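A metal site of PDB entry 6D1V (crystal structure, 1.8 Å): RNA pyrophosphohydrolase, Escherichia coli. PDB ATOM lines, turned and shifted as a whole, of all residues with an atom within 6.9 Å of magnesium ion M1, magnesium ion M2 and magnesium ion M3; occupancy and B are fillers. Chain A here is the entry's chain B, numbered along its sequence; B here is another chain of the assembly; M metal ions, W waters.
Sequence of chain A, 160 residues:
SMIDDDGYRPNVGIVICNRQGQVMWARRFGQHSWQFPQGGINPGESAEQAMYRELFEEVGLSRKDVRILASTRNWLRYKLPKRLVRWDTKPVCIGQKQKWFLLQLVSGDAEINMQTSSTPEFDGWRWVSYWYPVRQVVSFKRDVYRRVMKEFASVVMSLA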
ATOM      1  N   ARG A   9      -9.857   3.213  14.216  1.00  0.00           N
ATOM      2  CA  ARG A   9      -9.172   2.526  13.131  1.00  0.00           C
ATOM      3  C   ARG A   9      -8.999   1.051  13.470  1.00  0.00           C
ATOM      4  O   ARG A   9      -8.482   0.724  14.553  1.00  0.00           O
ATOM      5  CB  ARG A   9      -7.809   3.177  12.870  1.00  0.00           C
ATOM      6  CG  ARG A   9      -7.127   2.704  11.598  1.00  0.00           C
ATOM      7  CD  ARG A   9      -5.813   3.437  11.387  1.00  0.00           C
ATOM      8  NE  ARG A   9      -4.806   2.959  12.330  1.00  0.00           N
ATOM      9  CZ  ARG A   9      -3.510   2.882  12.076  1.00  0.00           C
ATOM     10  NH1 ARG A   9      -3.029   3.249  10.896  1.00  0.00           N
ATOM     11  NH2 ARG A   9      -2.689   2.423  13.027  1.00  0.00           N
ATOM     12  N   ASN A  11      -7.190  -2.446  13.662  1.00  0.00           N
ATOM     13  CA  ASN A  11      -5.782  -2.488  14.040  1.00  0.00           C
ATOM     14  C   ASN A  11      -5.464  -3.893  14.549  1.00  0.00           C
ATOM     15  O   ASN A  11      -6.357  -4.574  15.059  1.00  0.00           O
ATOM     16  CB  ASN A  11      -5.514  -1.387  15.092  1.00  0.00           C
ATOM     17  CG  ASN A  11      -4.080  -1.365  15.597  1.00  0.00           C
ATOM     18  OD1 ASN A  11      -3.644  -2.283  16.311  1.00  0.00           O
ATOM     19  ND2 ASN A  11      -3.358  -0.286  15.289  1.00  0.00           N
ATOM     20  N   VAL A  12      -4.213  -4.338  14.373  1.00  0.00           N
ATOM     21  CA  VAL A  12      -3.765  -5.622  14.916  1.00  0.00           C
ATOM     22  C   VAL A  12      -2.583  -5.386  15.848  1.00  0.00           C
ATOM     23  O   VAL A  12      -1.686  -4.591  15.550  1.00  0.00           O
ATOM     24  CB  VAL A  12      -3.374  -6.648  13.831  1.00  0.00           C
ATOM     25  CG1 VAL A  12      -4.599  -7.029  12.998  1.00  0.00           C
ATOM     26  CG2 VAL A  12      -2.252  -6.118  12.968  1.00  0.00           C
ATOM     27  N   GLN A  35       6.514  -0.646  23.832  1.00  0.00           N
ATOM     28  CA  GLN A  35       5.169  -1.171  23.610  1.00  0.00           C
ATOM     29  C   GLN A  35       5.301  -2.472  22.826  1.00  0.00           C
ATOM     30  O   GLN A  35       6.380  -2.825  22.359  1.00  0.00           O
ATOM     31  CB  GLN A  35       4.321  -0.178  22.823  1.00  0.00           C
ATOM     32  CG  GLN A  35       4.885  -0.061  21.376  1.00  0.00           C
ATOM     33  CD  GLN A  35       4.068   0.869  20.486  1.00  0.00           C
ATOM     34  OE1 GLN A  35       4.313   2.061  20.415  1.00  0.00           O
ATOM     35  NE2 GLN A  35       3.113   0.310  19.761  1.00  0.00           N
ATOM     36  N   PHE A  36       4.159  -3.149  22.667  1.00  0.00           N
ATOM     37  CA  PHE A  36       4.105  -4.257  21.724  1.00  0.00           C
ATOM     38  C   PHE A  36       3.909  -3.706  20.313  1.00  0.00           C
ATOM     39  O   PHE A  36       3.296  -2.641  20.145  1.00  0.00           O
ATOM     40  CB  PHE A  36       2.924  -5.157  22.045  1.00  0.00           C
ATOM     41  CG  PHE A  36       3.066  -6.001  23.294  1.00  0.00           C
ATOM     42  CD1 PHE A  36       4.237  -6.683  23.580  1.00  0.00           C
ATOM     43  CD2 PHE A  36       1.964  -6.185  24.132  1.00  0.00           C
ATOM     44  CE1 PHE A  36       4.344  -7.497  24.704  1.00  0.00           C
ATOM     45  CE2 PHE A  36       2.049  -7.027  25.260  1.00  0.00           C
ATOM     46  CZ  PHE A  36       3.223  -7.668  25.550  1.00  0.00           C
ATOM     47  N   PRO A  37       4.373  -4.415  19.283  1.00  0.00           N
ATOM     48  CA  PRO A  37       4.053  -4.014  17.902  1.00  0.00           C
ATOM     49  C   PRO A  37       2.553  -4.019  17.673  1.00  0.00           C
ATOM     50  O   PRO A  37       1.838  -4.927  18.128  1.00  0.00           O
ATOM     51  CB  PRO A  37       4.731  -5.085  17.035  1.00  0.00           C
ATOM     52  CG  PRO A  37       5.812  -5.716  17.928  1.00  0.00           C
ATOM     53  CD  PRO A  37       5.229  -5.615  19.337  1.00  0.00           C
ATOM     54  N   GLN A  38       2.082  -3.029  16.918  1.00  0.00           N
ATOM     55  CA  GLN A  38       0.711  -2.983  16.417  1.00  0.00           C
ATOM     56  C   GLN A  38       0.679  -2.145  15.143  1.00  0.00           C
ATOM     57  O   GLN A  38       1.563  -1.320  14.904  1.00  0.00           O
ATOM     58  CB  GLN A  38      -0.265  -2.377  17.423  1.00  0.00           C
ATOM     59  CG  GLN A  38       0.104  -0.977  17.842  1.00  0.00           C
ATOM     60  CD  GLN A  38      -0.901  -0.386  18.789  1.00  0.00           C
ATOM     61  OE1 GLN A  38      -1.108  -0.897  19.896  1.00  0.00           O
ATOM     62  NE2 GLN A  38      -1.550   0.695  18.371  1.00  0.00           N
ATOM     63  N   GLY A  39      -0.390  -2.311  14.363  1.00  0.00           N
ATOM     64  CA  GLY A  39      -0.462  -1.619  13.078  1.00  0.00           C
ATOM     65  C   GLY A  39      -1.861  -1.615  12.499  1.00  0.00           C
ATOM     66  O   GLY A  39      -2.690  -2.479  12.826  1.00  0.00           O
ATOM     67  N   GLY A  40      -2.112  -0.623  11.654  1.00  0.00           N
ATOM     68  CA  GLY A  40      -3.441  -0.466  11.058  1.00  0.00           C
ATOM     69  C   GLY A  40      -3.704  -1.517   9.987  1.00  0.00           C
ATOM     70  O   GLY A  40      -2.814  -1.895   9.212  1.00  0.00           O
ATOM     71  N   ILE A  41      -4.942  -2.008   9.963  1.00  0.00           N
ATOM     72  CA  ILE A  41      -5.400  -2.933   8.931  1.00  0.00           C
ATOM     73  C   ILE A  41      -5.735  -2.142   7.674  1.00  0.00           C
ATOM     74  O   ILE A  41      -6.406  -1.104   7.738  1.00  0.00           O
ATOM     75  CB  ILE A  41      -6.610  -3.734   9.418  1.00  0.00           C
ATOM     76  CG1 ILE A  41      -6.213  -4.661  10.559  1.00  0.00           C
ATOM     77  CG2 ILE A  41      -7.226  -4.532   8.264  1.00  0.00           C
ATOM     78  CD1 ILE A  41      -7.355  -5.503  11.131  1.00  0.00           C
ATOM     79  N   ASN A  42      -5.257  -2.613   6.526  1.00  0.00           N
ATOM     80  CA  ASN A  42      -5.408  -1.861   5.292  1.00  0.00           C
ATOM     81  C   ASN A  42      -6.672  -2.267   4.546  1.00  0.00           C
ATOM     82  O   ASN A  42      -7.195  -3.380   4.747  1.00  0.00           O
ATOM     83  CB  ASN A  42      -4.176  -2.062   4.416  1.00  0.00           C
ATOM     84  CG  ASN A  42      -3.082  -1.092   4.766  1.00  0.00           C
ATOM     85  OD1 ASN A  42      -3.341   0.022   5.205  1.00  0.00           O
ATOM     86  ND2 ASN A  42      -1.835  -1.519   4.603  1.00  0.00           N
ATOM     87  N   ARG A  53       1.968  -8.588   7.738  1.00  0.00           N
ATOM     88  CA  ARG A  53       2.540  -7.418   7.078  1.00  0.00           C
ATOM     89  C   ARG A  53       3.249  -6.494   8.068  1.00  0.00           C
ATOM     90  O   ARG A  53       4.390  -6.099   7.849  1.00  0.00           O
ATOM     91  CB  ARG A  53       1.455  -6.652   6.325  1.00  0.00           C
ATOM     92  CG  ARG A  53       1.961  -5.418   5.586  1.00  0.00           C
ATOM     93  CD  ARG A  53       0.856  -4.747   4.801  1.00  0.00           C
ATOM     94  NE  ARG A  53      -0.184  -4.204   5.676  1.00  0.00           N
ATOM     95  CZ  ARG A  53      -0.104  -3.026   6.277  1.00  0.00           C
ATOM     96  NH1 ARG A  53      -1.092  -2.604   7.054  1.00  0.00           N
ATOM     97  NH2 ARG A  53       0.966  -2.253   6.100  1.00  0.00           N
ATOM     98  N   GLU A  54       2.561  -6.155   9.160  1.00  0.00           N
ATOM     99  CA  GLU A  54       3.141  -5.272  10.167  1.00  0.00           C
ATOM    100  C   GLU A  54       4.237  -5.988  10.955  1.00  0.00           C
ATOM    101  O   GLU A  54       5.200  -5.360  11.385  1.00  0.00           O
ATOM    102  CB  GLU A  54       2.049  -4.750  11.102  1.00  0.00           C
ATOM    103  CG  GLU A  54       1.057  -3.773  10.452  1.00  0.00           C
ATOM    104  CD  GLU A  54       1.529  -2.326  10.392  1.00  0.00           C
ATOM    105  OE1 GLU A  54       2.520  -1.953  11.066  1.00  0.00           O
ATOM    106  OE2 GLU A  54       0.890  -1.555   9.647  1.00  0.00           O
ATOM    107  N   GLU A  57       7.243  -5.673   8.827  1.00  0.00           N
ATOM    108  CA  GLU A  57       7.585  -4.252   8.746  1.00  0.00           C
ATOM    109  C   GLU A  57       8.232  -3.727  10.035  1.00  0.00           C
ATOM    110  O   GLU A  57       9.196  -2.954   9.997  1.00  0.00           O
ATOM    111  CB  GLU A  57       6.328  -3.454   8.435  1.00  0.00           C
ATOM    112  CG  GLU A  57       6.449  -1.955   8.606  1.00  0.00           C
ATOM    113  CD  GLU A  57       5.135  -1.329   9.062  1.00  0.00           C
ATOM    114  OE1 GLU A  57       5.035  -0.922  10.257  1.00  0.00           O
ATOM    115  OE2 GLU A  57       4.197  -1.257   8.199  1.00  0.00           O
ATOM    116  N   GLU A  58       7.721  -4.147  11.189  1.00  0.00           N
ATOM    117  CA  GLU A  58       8.133  -3.584  12.485  1.00  0.00           C
ATOM    118  C   GLU A  58       9.189  -4.412  13.191  1.00  0.00           C
ATOM    119  O   GLU A  58      10.031  -3.840  13.895  1.00  0.00           O
ATOM    120  CB  GLU A  58       6.900  -3.448  13.405  1.00  0.00           C
ATOM    121  CG  GLU A  58       5.845  -2.511  12.806  1.00  0.00           C
ATOM    122  CD  GLU A  58       4.850  -1.979  13.814  1.00  0.00           C
ATOM    123  OE1 GLU A  58       4.877  -2.402  14.997  1.00  0.00           O
ATOM    124  OE2 GLU A  58       4.030  -1.127  13.429  1.00  0.00           O
ATOM    125  N   GLU A 121       9.358   1.949  13.054  1.00  0.00           N
ATOM    126  CA  GLU A 121       8.629   2.441  14.213  1.00  0.00           C
ATOM    127  C   GLU A 121       9.381   2.169  15.509  1.00  0.00           C
ATOM    128  O   GLU A 121       9.112   2.829  16.515  1.00  0.00           O
ATOM    129  CB  GLU A 121       7.234   1.817  14.269  1.00  0.00           C
ATOM    130  CG  GLU A 121       6.302   2.449  13.265  1.00  0.00           C
ATOM    131  CD  GLU A 121       5.003   1.690  13.112  1.00  0.00           C
ATOM    132  OE1 GLU A 121       4.249   1.536  14.126  1.00  0.00           O
ATOM    133  OE2 GLU A 121       4.749   1.253  11.961  1.00  0.00           O
ATOM    134  N   PHE A 122      10.340   1.250  15.505  1.00  0.00           N
ATOM    135  CA  PHE A 122      11.090   0.886  16.692  1.00  0.00           C
ATOM    136  C   PHE A 122      12.580   0.924  16.432  1.00  0.00           C
ATOM    137  O   PHE A 122      13.041   0.733  15.300  1.00  0.00           O
ATOM    138  CB  PHE A 122      10.718  -0.509  17.140  1.00  0.00           C
ATOM    139  CG  PHE A 122       9.281  -0.697  17.477  1.00  0.00           C
ATOM    140  CD1 PHE A 122       8.669   0.108  18.437  1.00  0.00           C
ATOM    141  CD2 PHE A 122       8.544  -1.683  16.850  1.00  0.00           C
ATOM    142  CE1 PHE A 122       7.322  -0.073  18.756  1.00  0.00           C
ATOM    143  CE2 PHE A 122       7.192  -1.869  17.175  1.00  0.00           C
ATOM    144  CZ  PHE A 122       6.597  -1.066  18.118  1.00  0.00           C
ATOM    145  PG  APC B   1       0.385   2.120  15.035  1.00  0.00           P
ATOM    146  O1G APC B   1      -0.921   1.762  15.757  1.00  0.00           O
ATOM    147  O2G APC B   1       0.789   3.553  15.157  1.00  0.00           O
ATOM    148  O3G APC B   1       1.602   1.299  15.336  1.00  0.00           O
ATOM    149  PB  APC B   1       0.918   1.543  12.207  1.00  0.00           P
ATOM    150  O1B APC B   1       0.044   0.896  11.033  1.00  0.00           O
ATOM    151  O2B APC B   1       1.929   0.560  12.626  1.00  0.00           O
ATOM    152  O3B APC B   1      -0.051   1.873  13.468  1.00  0.00           O
ATOM    153  PA  APC B   1       0.617   4.458  11.479  1.00  0.00           P
ATOM    154  O1A APC B   1      -0.466   4.122  10.334  1.00  0.00           O
ATOM    155  O2A APC B   1       1.468   5.611  11.083  1.00  0.00           O
ATOM    156  C3A APC B   1       1.775   3.058  11.721  1.00  0.00           C
ATOM    157  O5' APC B   1      -0.110   4.790  12.901  1.00  0.00           O
ATOM    158  C5' APC B   1       0.331   5.920  13.662  1.00  0.00           C
ATOM    159  C4' APC B   1      -0.585   6.274  14.832  1.00  0.00           C
ATOM    160  O4' APC B   1      -0.941   7.607  14.520  1.00  0.00           O
ATOM    161  C3' APC B   1      -1.896   5.496  14.877  1.00  0.00           C
ATOM    162  O3' APC B   1      -2.519   5.700  16.152  1.00  0.00           O
ATOM    163  C2' APC B   1      -2.730   6.194  13.815  1.00  0.00           C
ATOM    164  O2' APC B   1      -4.145   6.158  14.052  1.00  0.00           O
ATOM    165  C1' APC B   1      -2.243   7.623  13.917  1.00  0.00           C
ATOM    166  N9  APC B   1      -2.216   8.243  12.573  1.00  0.00           N
ATOM    167  C8  APC B   1      -1.909   7.652  11.401  1.00  0.00           C
ATOM    168  N7  APC B   1      -2.014   8.534  10.367  1.00  0.00           N
ATOM    169  C5  APC B   1      -2.394   9.724  10.895  1.00  0.00           C
ATOM    170  C6  APC B   1      -2.683  11.082  10.392  1.00  0.00           C
ATOM    171  N6  APC B   1      -2.578  11.358   9.057  1.00  0.00           N
ATOM    172  N1  APC B   1      -3.048  12.031  11.293  1.00  0.00           N
ATOM    173  C2  APC B   1      -3.150  11.764  12.605  1.00  0.00           C
ATOM    174  N3  APC B   1      -2.903  10.556  13.138  1.00  0.00           N
ATOM    175  C4  APC B   1      -2.533   9.513  12.346  1.00  0.00           C
ATOM    176  P     G B   2      -1.867   5.160  17.522  1.00  0.00           P
ATOM    177  OP1   G B   2      -1.016   3.973  17.240  1.00  0.00           O
ATOM    178  OP2   G B   2      -2.955   5.062  18.526  1.00  0.00           O
ATOM    179  O5'   G B   2      -0.915   6.352  17.961  1.00  0.00           O
ATOM    180  C5'   G B   2      -1.453   7.632  18.224  1.00  0.00           C
ATOM    181  C4'   G B   2      -0.531   8.433  19.098  1.00  0.00           C
ATOM    182  O4'   G B   2      -0.635   7.944  20.457  1.00  0.00           O
ATOM    183  C3'   G B   2       0.947   8.295  18.765  1.00  0.00           C
ATOM    184  O3'   G B   2       1.366   9.161  17.735  1.00  0.00           O
ATOM    185  C2'   G B   2       1.635   8.535  20.105  1.00  0.00           C
ATOM    186  O2'   G B   2       1.706   9.926  20.398  1.00  0.00           O
ATOM    187  C1'   G B   2       0.645   7.901  21.063  1.00  0.00           C
ATOM    188  N9    G B   2       0.930   6.522  21.299  1.00  0.00           N
ATOM    189  C8    G B   2       0.345   5.407  20.702  1.00  0.00           C
ATOM    190  N7    G B   2       0.803   4.280  21.186  1.00  0.00           N
ATOM    191  C5    G B   2       1.717   4.647  22.187  1.00  0.00           C
ATOM    192  C6    G B   2       2.504   3.862  23.067  1.00  0.00           C
ATOM    193  O6    G B   2       2.545   2.611  23.164  1.00  0.00           O
ATOM    194  N1    G B   2       3.272   4.664  23.902  1.00  0.00           N
ATOM    195  C2    G B   2       3.297   6.040  23.908  1.00  0.00           C
ATOM    196  N2    G B   2       4.117   6.608  24.799  1.00  0.00           N
ATOM    197  N3    G B   2       2.562   6.789  23.099  1.00  0.00           N
ATOM    198  C4    G B   2       1.806   6.029  22.279  1.00  0.00           C
HETATM  199 MG    MG M   1       2.806   0.129  14.408  1.00  0.00          MG
HETATM  200 MG    MG M   2       0.787   0.385   9.219  1.00  0.00          MG
HETATM  201 MG    MG M   3       3.474  -0.249  11.517  1.00  0.00          MG
HETATM  202  O   HOH W   1       1.756   0.056   7.208  1.00  0.00           O
HETATM  203  O   HOH W   2       3.831  -0.188  16.267  1.00  0.00           O
HETATM  204  O   HOH W   3      -1.174  -0.092   8.649  1.00  0.00           O
HETATM  205  O   HOH W   4       2.792   0.721   9.669  1.00  0.00           O
HETATM  206  O   HOH W   5       0.475   2.506   8.567  1.00  0.00           O
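O1A of APC 1 of chain B is in salt-bridge range of the guanidinium group (NH1) of Arg 9 (2.8 Å). The side-chain amide nitrogen (ND2) of Asn 11 sits close to the backbone carbonyl oxygen (O) of Gly 39 (3.4 Å). The backbone carbonyl oxygen (O) of Gly 39 sits at hydrogen-bond distance from the backbone NH (N) of Val 12. The backbone carbonyl oxygen (O) of Gly 40 sits at hydrogen-bond distance from the guanidinium group (NH1) of Arg 53 (2.9 Å). N of Gly 40 lies close to O1B of APC 1 of chain B, 2.7 Å away. The guanidinium group (NH1) of Arg 53 lies close to the side-chain carboxylate (OE2) of Glu 54 (3.4 Å). The side-chain amide nitrogen (ND2) of Asn 11 is in hydrogen-bond range of O1G of APC 1 of chain B (3.2 Å). NH2 of Arg 53 lies within salt-bridge range of OE2 of Glu 57 (3.98 Å).
Merely in contact with magnesium ion M1: Gly 39. Of the 19 residues printed, 6 come within 4 Å of magnesium ion M1.
Residues that only touch magnesium ion M2: Gly 40. Of the 19 residues printed, 4 come within 4 Å of magnesium ion M2.
Of the 19 residues printed, 5 come within 4 Å of magnesium ion M3.
Magnesium ion M1 is bound by O3G of APC 1 of chain B, O of Gln 38, OE2 of Glu 58, O2B of APC 1 of chain B, OE1 of Glu 121 and water W2.
Magnesium ion M2 is bound by OE2 of Glu 54 (2.0 Å). Magnesium ion M2 is bound by O1B of APC 1 of chain B. Magnesium ion M2 is bound by water W4, at 2.1 Å. Water W3 binds magnesium ion M2 (2.1 Å). Water W5 binds magnesium ion M2 (2.2 Å). Water W1 binds magnesium ion M2 (2.3 Å). Magnesium ion M2 has six donor atoms within binding distance.
Magnesium ion M3 is bound by OE1 of Glu 54, at 2.0 Å. The side-chain carboxylate (OE2) of Glu 121 is bound to magnesium ion M3 (2.0 Å). O2B of APC 1 of chain B is bound to magnesium ion M3. Magnesium ion M3 is bound by the side-chain carboxylate (OE1) of Glu 57 (2.1 Å). OE2 of Glu 58 binds magnesium ion M3, at 2.2 Å. Water W4 is bound to magnesium ion M3 (2.2 Å).
Water W2 lies within hydrogen-bond range of the side-chain carboxylate of Glu 58 (2.8 Å) and the backbone NH of Gln 38 (3.4 Å). Water W3 lies within hydrogen-bond range of the backbone carbonyl oxygen (O) of Gly 40 (2.5 Å) and the guanidinium group (NH1) of Arg 53 (3.0 Å). Water W1 bridges NH2 of Arg 53 (2.7 Å) and OE2 of Glu 57 (2.9 Å).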
